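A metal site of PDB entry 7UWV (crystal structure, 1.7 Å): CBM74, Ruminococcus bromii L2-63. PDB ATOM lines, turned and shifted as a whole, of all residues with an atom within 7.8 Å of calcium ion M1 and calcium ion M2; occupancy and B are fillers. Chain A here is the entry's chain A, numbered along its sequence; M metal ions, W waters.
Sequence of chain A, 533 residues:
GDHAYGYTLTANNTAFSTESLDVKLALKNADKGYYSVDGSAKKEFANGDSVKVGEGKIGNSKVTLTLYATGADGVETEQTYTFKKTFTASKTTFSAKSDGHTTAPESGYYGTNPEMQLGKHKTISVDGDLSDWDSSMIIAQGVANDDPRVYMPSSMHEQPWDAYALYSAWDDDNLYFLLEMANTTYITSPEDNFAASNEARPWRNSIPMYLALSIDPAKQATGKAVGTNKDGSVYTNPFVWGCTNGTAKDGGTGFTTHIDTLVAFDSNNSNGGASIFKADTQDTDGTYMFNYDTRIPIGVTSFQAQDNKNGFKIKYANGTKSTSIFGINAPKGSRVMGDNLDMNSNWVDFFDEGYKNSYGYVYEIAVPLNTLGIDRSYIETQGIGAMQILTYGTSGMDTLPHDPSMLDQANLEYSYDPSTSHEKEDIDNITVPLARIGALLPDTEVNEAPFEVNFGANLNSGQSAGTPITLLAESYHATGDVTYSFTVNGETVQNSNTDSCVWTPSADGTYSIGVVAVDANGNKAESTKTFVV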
ATOM      1  N   PRO A 148      14.797  -0.067  20.313  1.00  0.00           N
ATOM      2  CA  PRO A 148      15.579  -0.550  21.453  1.00  0.00           C
ATOM      3  C   PRO A 148      17.111  -0.634  21.282  1.00  0.00           C
ATOM      4  O   PRO A 148      17.816  -0.445  22.268  1.00  0.00           O
ATOM      5  CB  PRO A 148      14.998  -1.950  21.689  1.00  0.00           C
ATOM      6  CG  PRO A 148      13.549  -1.785  21.263  1.00  0.00           C
ATOM      7  CD  PRO A 148      13.672  -0.964  19.996  1.00  0.00           C
ATOM      8  N   ASP A 250      10.838 -16.807  23.550  1.00  0.00           N
ATOM      9  CA  ASP A 250      11.424 -15.480  23.207  1.00  0.00           C
ATOM     10  C   ASP A 250      10.317 -14.413  23.261  1.00  0.00           C
ATOM     11  O   ASP A 250      10.385 -13.439  22.501  1.00  0.00           O
ATOM     12  CB  ASP A 250      12.130 -15.548  21.859  1.00  0.00           C
ATOM     13  CG  ASP A 250      13.285 -16.543  21.838  1.00  0.00           C
ATOM     14  OD1 ASP A 250      13.881 -16.786  22.913  1.00  0.00           O
ATOM     15  OD2 ASP A 250      13.570 -17.056  20.746  1.00  0.00           O
ATOM     16  N   GLY A 251       9.345 -14.603  24.163  1.00  0.00           N
ATOM     17  CA  GLY A 251       8.381 -13.551  24.537  1.00  0.00           C
ATOM     18  C   GLY A 251       7.397 -13.216  23.426  1.00  0.00           C
ATOM     19  O   GLY A 251       7.154 -14.060  22.544  1.00  0.00           O
ATOM     20  N   GLY A 252       6.851 -12.003  23.472  1.00  0.00           N
ATOM     21  CA  GLY A 252       5.696 -11.590  22.677  1.00  0.00           C
ATOM     22  C   GLY A 252       5.098 -10.314  23.231  1.00  0.00           C
ATOM     23  O   GLY A 252       5.698  -9.741  24.173  1.00  0.00           O
ATOM     24  N   THR A 253       3.968  -9.888  22.676  1.00  0.00           N
ATOM     25  CA  THR A 253       3.251  -8.650  23.072  1.00  0.00           C
ATOM     26  C   THR A 253       1.859  -9.038  23.582  1.00  0.00           C
ATOM     27  O   THR A 253       1.113  -9.666  22.813  1.00  0.00           O
ATOM     28  CB  THR A 253       3.185  -7.639  21.927  1.00  0.00           C
ATOM     29  OG1 THR A 253       4.520  -7.428  21.468  1.00  0.00           O
ATOM     30  CG2 THR A 253       2.546  -6.337  22.343  1.00  0.00           C
ATOM     31  N   LEU A 390       5.719  -3.266  15.578  1.00  0.00           N
ATOM     32  CA  LEU A 390       6.912  -3.863  14.934  1.00  0.00           C
ATOM     33  C   LEU A 390       7.567  -4.833  15.902  1.00  0.00           C
ATOM     34  O   LEU A 390       7.538  -4.590  17.122  1.00  0.00           O
ATOM     35  CB  LEU A 390       7.910  -2.763  14.558  1.00  0.00           C
ATOM     36  CG  LEU A 390       7.420  -1.731  13.542  1.00  0.00           C
ATOM     37  CD1 LEU A 390       8.547  -0.775  13.222  1.00  0.00           C
ATOM     38  CD2 LEU A 390       6.910  -2.405  12.274  1.00  0.00           C
ATOM     39  N   THR A 391       8.173  -5.881  15.361  1.00  0.00           N
ATOM     40  CA  THR A 391       8.966  -6.885  16.091  1.00  0.00           C
ATOM     41  C   THR A 391      10.305  -7.069  15.379  1.00  0.00           C
ATOM     42  O   THR A 391      10.504  -6.491  14.284  1.00  0.00           O
ATOM     43  CB  THR A 391       8.235  -8.230  16.174  1.00  0.00           C
ATOM     44  OG1 THR A 391       8.383  -8.908  14.928  1.00  0.00           O
ATOM     45  CG2 THR A 391       6.762  -8.093  16.519  1.00  0.00           C
ATOM     46  N   THR A 394       9.560 -11.916  17.374  1.00  0.00           N
ATOM     47  CA  THR A 394       8.610 -12.342  18.438  1.00  0.00           C
ATOM     48  C   THR A 394       8.104 -11.110  19.184  1.00  0.00           C
ATOM     49  O   THR A 394       7.016 -10.610  18.828  1.00  0.00           O
ATOM     50  CB  THR A 394       9.256 -13.385  19.359  1.00  0.00           C
ATOM     51  OG1 THR A 394      10.476 -12.860  19.880  1.00  0.00           O
ATOM     52  CG2 THR A 394       9.506 -14.707  18.661  1.00  0.00           C
ATOM     53  N   SER A 395       8.894 -10.613  20.145  1.00  0.00           N
ATOM     54  CA  SER A 395       8.546  -9.482  21.046  1.00  0.00           C
ATOM     55  C   SER A 395       8.486  -8.161  20.258  1.00  0.00           C
ATOM     56  O   SER A 395       9.193  -8.012  19.235  1.00  0.00           O
ATOM     57  CB  SER A 395       9.517  -9.391  22.193  1.00  0.00           C
ATOM     58  OG  SER A 395       9.098  -8.437  23.173  1.00  0.00           O
ATOM     59  N   GLY A 396       7.723  -7.218  20.785  1.00  0.00           N
ATOM     60  CA  GLY A 396       7.622  -5.844  20.270  1.00  0.00           C
ATOM     61  C   GLY A 396       8.946  -5.100  20.364  1.00  0.00           C
ATOM     62  O   GLY A 396       9.734  -5.366  21.311  1.00  0.00           O
ATOM     63  N   MET A 397       9.175  -4.191  19.419  1.00  0.00           N
ATOM     64  CA  MET A 397      10.354  -3.296  19.402  1.00  0.00           C
ATOM     65  C   MET A 397       9.897  -1.830  19.365  1.00  0.00           C
ATOM     66  O   MET A 397      10.596  -0.997  19.975  1.00  0.00           O
ATOM     67  CB  MET A 397      11.231  -3.583  18.175  1.00  0.00           C
ATOM     68  CG  MET A 397      11.769  -5.007  18.164  1.00  0.00           C
ATOM     69  SD  MET A 397      13.092  -5.215  19.379  1.00  0.00           S
ATOM     70  CE  MET A 397      14.503  -4.626  18.453  1.00  0.00           C
ATOM     71  N   ASP A 398       8.813  -1.515  18.657  1.00  0.00           N
ATOM     72  CA  ASP A 398       8.303  -0.129  18.504  1.00  0.00           C
ATOM     73  C   ASP A 398       6.806  -0.240  18.194  1.00  0.00           C
ATOM     74  O   ASP A 398       6.408  -1.231  17.579  1.00  0.00           O
ATOM     75  CB  ASP A 398       9.086   0.649  17.435  1.00  0.00           C
ATOM     76  CG  ASP A 398       8.967   2.174  17.496  1.00  0.00           C
ATOM     77  OD1 ASP A 398       8.097   2.665  18.231  1.00  0.00           O
ATOM     78  OD2 ASP A 398       9.735   2.865  16.757  1.00  0.00           O
ATOM     79  N   ASP A 403       4.411   2.954  23.210  1.00  0.00           N
ATOM     80  CA  ASP A 403       4.141   2.385  24.550  1.00  0.00           C
ATOM     81  C   ASP A 403       5.482   2.178  25.258  1.00  0.00           C
ATOM     82  O   ASP A 403       6.414   1.651  24.656  1.00  0.00           O
ATOM     83  CB  ASP A 403       3.330   1.103  24.427  1.00  0.00           C
ATOM     84  CG  ASP A 403       2.853   0.549  25.759  1.00  0.00           C
ATOM     85  OD1 ASP A 403       1.629   0.632  26.025  1.00  0.00           O
ATOM     86  OD2 ASP A 403       3.711   0.036  26.514  1.00  0.00           O
ATOM     87  N   PRO A 404       5.608   2.580  26.541  1.00  0.00           N
ATOM     88  CA  PRO A 404       6.885   2.494  27.252  1.00  0.00           C
ATOM     89  C   PRO A 404       7.382   1.056  27.466  1.00  0.00           C
ATOM     90  O   PRO A 404       8.561   0.908  27.727  1.00  0.00           O
ATOM     91  CB  PRO A 404       6.600   3.174  28.598  1.00  0.00           C
ATOM     92  CG  PRO A 404       5.097   3.063  28.776  1.00  0.00           C
ATOM     93  CD  PRO A 404       4.537   3.142  27.381  1.00  0.00           C
ATOM     94  N   SER A 405       6.515   0.056  27.312  1.00  0.00           N
ATOM     95  CA  SER A 405       6.910  -1.376  27.424  1.00  0.00           C
ATOM     96  C   SER A 405       7.841  -1.757  26.259  1.00  0.00           C
ATOM     97  O   SER A 405       8.502  -2.806  26.331  1.00  0.00           O
ATOM     98  CB  SER A 405       5.709  -2.294  27.494  1.00  0.00           C
ATOM     99  OG  SER A 405       5.007  -2.311  26.262  1.00  0.00           O
ATOM    100  N   MET A 406       7.932  -0.912  25.231  1.00  0.00           N
ATOM    101  CA  MET A 406       8.882  -1.132  24.116  1.00  0.00           C
ATOM    102  C   MET A 406      10.324  -0.846  24.563  1.00  0.00           C
ATOM    103  O   MET A 406      11.241  -1.316  23.863  1.00  0.00           O
ATOM    104  CB  MET A 406       8.548  -0.262  22.903  1.00  0.00           C
ATOM    105  CG  MET A 406       7.243  -0.632  22.228  1.00  0.00           C
ATOM    106  SD  MET A 406       7.159  -2.364  21.669  1.00  0.00           S
ATOM    107  CE  MET A 406       5.908  -2.973  22.794  1.00  0.00           C
ATOM    108  N   LEU A 407      10.538  -0.100  25.659  1.00  0.00           N
ATOM    109  CA  LEU A 407      11.900   0.366  26.052  1.00  0.00           C
ATOM    110  C   LEU A 407      12.251   0.012  27.494  1.00  0.00           C
ATOM    111  O   LEU A 407      13.366   0.376  27.919  1.00  0.00           O
ATOM    112  CB  LEU A 407      11.967   1.879  25.805  1.00  0.00           C
ATOM    113  CG  LEU A 407      11.948   2.269  24.330  1.00  0.00           C
ATOM    114  CD1 LEU A 407      11.959   3.789  24.145  1.00  0.00           C
ATOM    115  CD2 LEU A 407      13.106   1.636  23.584  1.00  0.00           C
ATOM    116  N   ASP A 408      11.386  -0.714  28.224  1.00  0.00           N
ATOM    117  CA  ASP A 408      11.595  -0.922  29.681  1.00  0.00           C
ATOM    118  C   ASP A 408      12.801  -1.839  29.922  1.00  0.00           C
ATOM    119  O   ASP A 408      13.345  -1.789  31.025  1.00  0.00           O
ATOM    120  CB  ASP A 408      10.327  -1.433  30.386  1.00  0.00           C
ATOM    121  CG  ASP A 408       9.811  -2.775  29.891  1.00  0.00           C
ATOM    122  OD1 ASP A 408      10.136  -3.155  28.765  1.00  0.00           O
ATOM    123  OD2 ASP A 408       9.059  -3.420  30.654  1.00  0.00           O
ATOM    124  N   GLN A 409      13.210  -2.627  28.924  1.00  0.00           N
ATOM    125  CA  GLN A 409      14.382  -3.531  29.052  1.00  0.00           C
ATOM    126  C   GLN A 409      15.341  -3.335  27.865  1.00  0.00           C
ATOM    127  O   GLN A 409      16.101  -4.261  27.574  1.00  0.00           O
ATOM    128  CB  GLN A 409      13.879  -4.968  29.206  1.00  0.00           C
ATOM    129  CG  GLN A 409      13.019  -5.147  30.459  1.00  0.00           C
ATOM    130  CD  GLN A 409      12.819  -6.598  30.824  1.00  0.00           C
ATOM    131  OE1 GLN A 409      13.542  -7.131  31.654  1.00  0.00           O
ATOM    132  NE2 GLN A 409      11.844  -7.237  30.205  1.00  0.00           N
ATOM    133  N   ALA A 410      15.342  -2.152  27.255  1.00  0.00           N
ATOM    134  CA  ALA A 410      16.086  -1.847  26.016  1.00  0.00           C
ATOM    135  C   ALA A 410      17.589  -2.016  26.244  1.00  0.00           C
ATOM    136  O   ALA A 410      18.259  -2.450  25.316  1.00  0.00           O
ATOM    137  CB  ALA A 410      15.757  -0.448  25.528  1.00  0.00           C
ATOM    138  N   SER A 421      19.678  -6.094  21.968  1.00  0.00           N
ATOM    139  CA  SER A 421      18.713  -5.733  23.038  1.00  0.00           C
ATOM    140  C   SER A 421      17.797  -6.895  23.432  1.00  0.00           C
ATOM    141  O   SER A 421      17.185  -7.519  22.550  1.00  0.00           O
ATOM    142  CB  SER A 421      17.891  -4.542  22.604  1.00  0.00           C
ATOM    143  OG  SER A 421      16.989  -4.165  23.630  1.00  0.00           O
ATOM    144  N   HIS A 422      17.636  -7.102  24.740  1.00  0.00           N
ATOM    145  CA  HIS A 422      16.648  -8.032  25.360  1.00  0.00           C
ATOM    146  C   HIS A 422      15.223  -7.711  24.892  1.00  0.00           C
ATOM    147  O   HIS A 422      14.368  -8.612  24.957  1.00  0.00           O
ATOM    148  CB  HIS A 422      16.772  -7.954  26.893  1.00  0.00           C
ATOM    149  CG  HIS A 422      15.901  -8.911  27.633  1.00  0.00           C
ATOM    150  ND1 HIS A 422      16.053 -10.277  27.521  1.00  0.00           N
ATOM    151  CD2 HIS A 422      14.913  -8.703  28.536  1.00  0.00           C
ATOM    152  CE1 HIS A 422      15.186 -10.882  28.307  1.00  0.00           C
ATOM    153  NE2 HIS A 422      14.472  -9.940  28.947  1.00  0.00           N
ATOM    154  N   GLU A 423      14.934  -6.488  24.441  1.00  0.00           N
ATOM    155  CA  GLU A 423      13.578  -6.143  23.938  1.00  0.00           C
ATOM    156  C   GLU A 423      13.153  -7.091  22.809  1.00  0.00           C
ATOM    157  O   GLU A 423      11.945  -7.174  22.533  1.00  0.00           O
ATOM    158  CB  GLU A 423      13.500  -4.682  23.479  1.00  0.00           C
ATOM    159  CG  GLU A 423      13.287  -3.725  24.630  1.00  0.00           C
ATOM    160  CD  GLU A 423      11.965  -3.906  25.365  1.00  0.00           C
ATOM    161  OE1 GLU A 423      11.049  -4.559  24.801  1.00  0.00           O
ATOM    162  OE2 GLU A 423      11.859  -3.402  26.502  1.00  0.00           O
ATOM    163  N   LYS A 424      14.107  -7.801  22.190  1.00  0.00           N
ATOM    164  CA  LYS A 424      13.801  -8.725  21.066  1.00  0.00           C
ATOM    165  C   LYS A 424      13.081  -9.971  21.586  1.00  0.00           C
ATOM    166  O   LYS A 424      12.423 -10.635  20.757  1.00  0.00           O
ATOM    167  CB  LYS A 424      15.080  -9.097  20.303  1.00  0.00           C
ATOM    168  CG  LYS A 424      15.704  -7.968  19.501  1.00  0.00           C
ATOM    169  CD  LYS A 424      16.785  -8.423  18.545  1.00  0.00           C
ATOM    170  CE  LYS A 424      17.961  -9.101  19.237  1.00  0.00           C
ATOM    171  NZ  LYS A 424      19.045  -9.424  18.283  1.00  0.00           N
ATOM    172  N   GLU A 425      13.226 -10.310  22.874  1.00  0.00           N
ATOM    173  CA  GLU A 425      12.837 -11.639  23.428  1.00  0.00           C
ATOM    174  C   GLU A 425      12.006 -11.517  24.711  1.00  0.00           C
ATOM    175  O   GLU A 425      11.710 -12.583  25.275  1.00  0.00           O
ATOM    176  CB  GLU A 425      14.096 -12.476  23.682  1.00  0.00           C
ATOM    177  CG  GLU A 425      14.926 -11.988  24.861  1.00  0.00           C
ATOM    178  CD  GLU A 425      16.235 -12.723  25.079  1.00  0.00           C
ATOM    179  OE1 GLU A 425      16.355 -13.887  24.625  1.00  0.00           O
ATOM    180  OE2 GLU A 425      17.154 -12.127  25.729  1.00  0.00           O
ATOM    181  N   ASP A 426      11.612 -10.316  25.141  1.00  0.00           N
ATOM    182  CA  ASP A 426      10.952 -10.108  26.465  1.00  0.00           C
ATOM    183  C   ASP A 426       9.438 -10.094  26.291  1.00  0.00           C
ATOM    184  O   ASP A 426       8.948 -10.185  25.144  1.00  0.00           O
ATOM    185  CB  ASP A 426      11.479  -8.852  27.168  1.00  0.00           C
ATOM    186  CG  ASP A 426      10.983  -7.545  26.578  1.00  0.00           C
ATOM    187  OD1 ASP A 426      10.720  -7.538  25.355  1.00  0.00           O
ATOM    188  OD2 ASP A 426      10.881  -6.530  27.339  1.00  0.00           O
ATOM    189  N   ILE A 427       8.695 -10.024  27.393  1.00  0.00           N
ATOM    190  CA  ILE A 427       7.208  -9.931  27.351  1.00  0.00           C
ATOM    191  C   ILE A 427       6.833  -8.462  27.484  1.00  0.00           C
ATOM    192  O   ILE A 427       7.153  -7.863  28.528  1.00  0.00           O
ATOM    193  CB  ILE A 427       6.533 -10.773  28.453  1.00  0.00           C
ATOM    194  CG1 ILE A 427       6.872 -12.260  28.308  1.00  0.00           C
ATOM    195  CG2 ILE A 427       5.031 -10.540  28.439  1.00  0.00           C
ATOM    196  CD1 ILE A 427       6.590 -13.066  29.543  1.00  0.00           C
ATOM    197  N   ASP A 428       6.215  -7.900  26.448  1.00  0.00           N
ATOM    198  CA  ASP A 428       5.691  -6.513  26.438  1.00  0.00           C
ATOM    199  C   ASP A 428       4.211  -6.556  26.833  1.00  0.00           C
ATOM    200  O   ASP A 428       3.550  -7.564  26.561  1.00  0.00           O
ATOM    201  CB  ASP A 428       5.884  -5.872  25.058  1.00  0.00           C
ATOM    202  CG  ASP A 428       7.328  -5.829  24.593  1.00  0.00           C
ATOM    203  OD1 ASP A 428       8.235  -5.765  25.466  1.00  0.00           O
ATOM    204  OD2 ASP A 428       7.548  -5.891  23.346  1.00  0.00           O
ATOM    205  N   ASN A 429       3.694  -5.494  27.449  1.00  0.00           N
ATOM    206  CA  ASN A 429       2.256  -5.389  27.777  1.00  0.00           C
ATOM    207  C   ASN A 429       1.784  -3.967  27.466  1.00  0.00           C
ATOM    208  O   ASN A 429       2.310  -3.032  28.096  1.00  0.00           O
ATOM    209  CB  ASN A 429       1.965  -5.810  29.215  1.00  0.00           C
ATOM    210  CG  ASN A 429       0.481  -5.915  29.478  1.00  0.00           C
ATOM    211  OD1 ASN A 429      -0.165  -4.909  29.762  1.00  0.00           O
ATOM    212  ND2 ASN A 429      -0.082  -7.113  29.380  1.00  0.00           N
HETATM  213 CA    CA M   1       9.651  -4.571  26.941  1.00  0.00          CA
HETATM  214 CA    CA M   2       9.951  -6.262  23.528  1.00  0.00          CA
HETATM  215  O   HOH W   1       8.157  -5.212  28.686  1.00  0.00           O
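The side-chain hydroxyl (OG) of Ser 405 is in hydrogen-bond range of the backbone carbonyl oxygen (O) of Asn 429 (3.3 Å).
OG of Ser 405 sits at hydrogen-bond distance from OD2 of Asp 403.
The side-chain carboxylate (OD2) of Asp 426 sits close to the side-chain amide nitrogen (NE2) of Gln 409, 3.1 Å away.
The backbone carbonyl oxygen (O) of Asp 426 is in hydrogen-bond range of the backbone NH (N) of Gly 252 (3.2 Å).
N of Asp 428 lies within hydrogen-bond range of O of Gly 252, 3.0 Å away.
The side-chain carboxylate of Glu 423 lies close to the backbone NH of Gln 409 (2.9 Å).
The backbone NH (N) of Glu 423 lies close to the side-chain hydroxyl (OG) of Ser 421.
N of Gly 396 lies within hydrogen-bond range of OG1 of Thr 253, 3.3 Å away.
Within 4 Å of calcium ion M1: Ser 405, Asp 408, Glu 423, Asp 426 and Asp 428.
The nearest printed residue that does not touch calcium ion M1 is Met 406 (4.4 Å).
Five residues have an atom within 4 Å of calcium ion M2: Ser 395, Gly 396, Glu 423, Asp 426 and Asp 428.
The nearest printed residue that does not touch calcium ion M2 is Lys 424 (4.6 Å).
O of Ser 405 is bound to calcium ion M1, at 2.2 Å.
Calcium ion M1 is bound by the side-chain carboxylate (OD2) of Asp 426.
The side-chain carboxylate (OD1) of Asp 408 binds calcium ion M1 (2.4 Å).
OD1 of Asp 428 binds calcium ion M1.
Calcium ion M1 is bound by water W1 (2.4 Å).
The side-chain carboxylate (OE2) of Glu 423 binds calcium ion M1, 2.5 Å away.
Calcium ion M1 is bound by OE1 of Glu 423.
Calcium ion M1 has seven donor atoms within binding distance.
Calcium ion M2 is bound by the side-chain carboxylate (OD1) of Asp 426, the side-chain hydroxyl (OG) of Ser 395, the side-chain carboxylate (OE1) of Glu 423, the backbone carbonyl oxygen (O) of Gly 396, the backbone carbonyl oxygen (O) of Glu 423, the side-chain carboxylate (OD2) of Asp 428 and the side-chain carboxylate (OD1) of Asp 428.
Water W1 bridges the side-chain carboxylate (OD2) of Asp 408 (2.8 Å) and the backbone carbonyl oxygen (O) of Ile 427 (2.8 Å).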
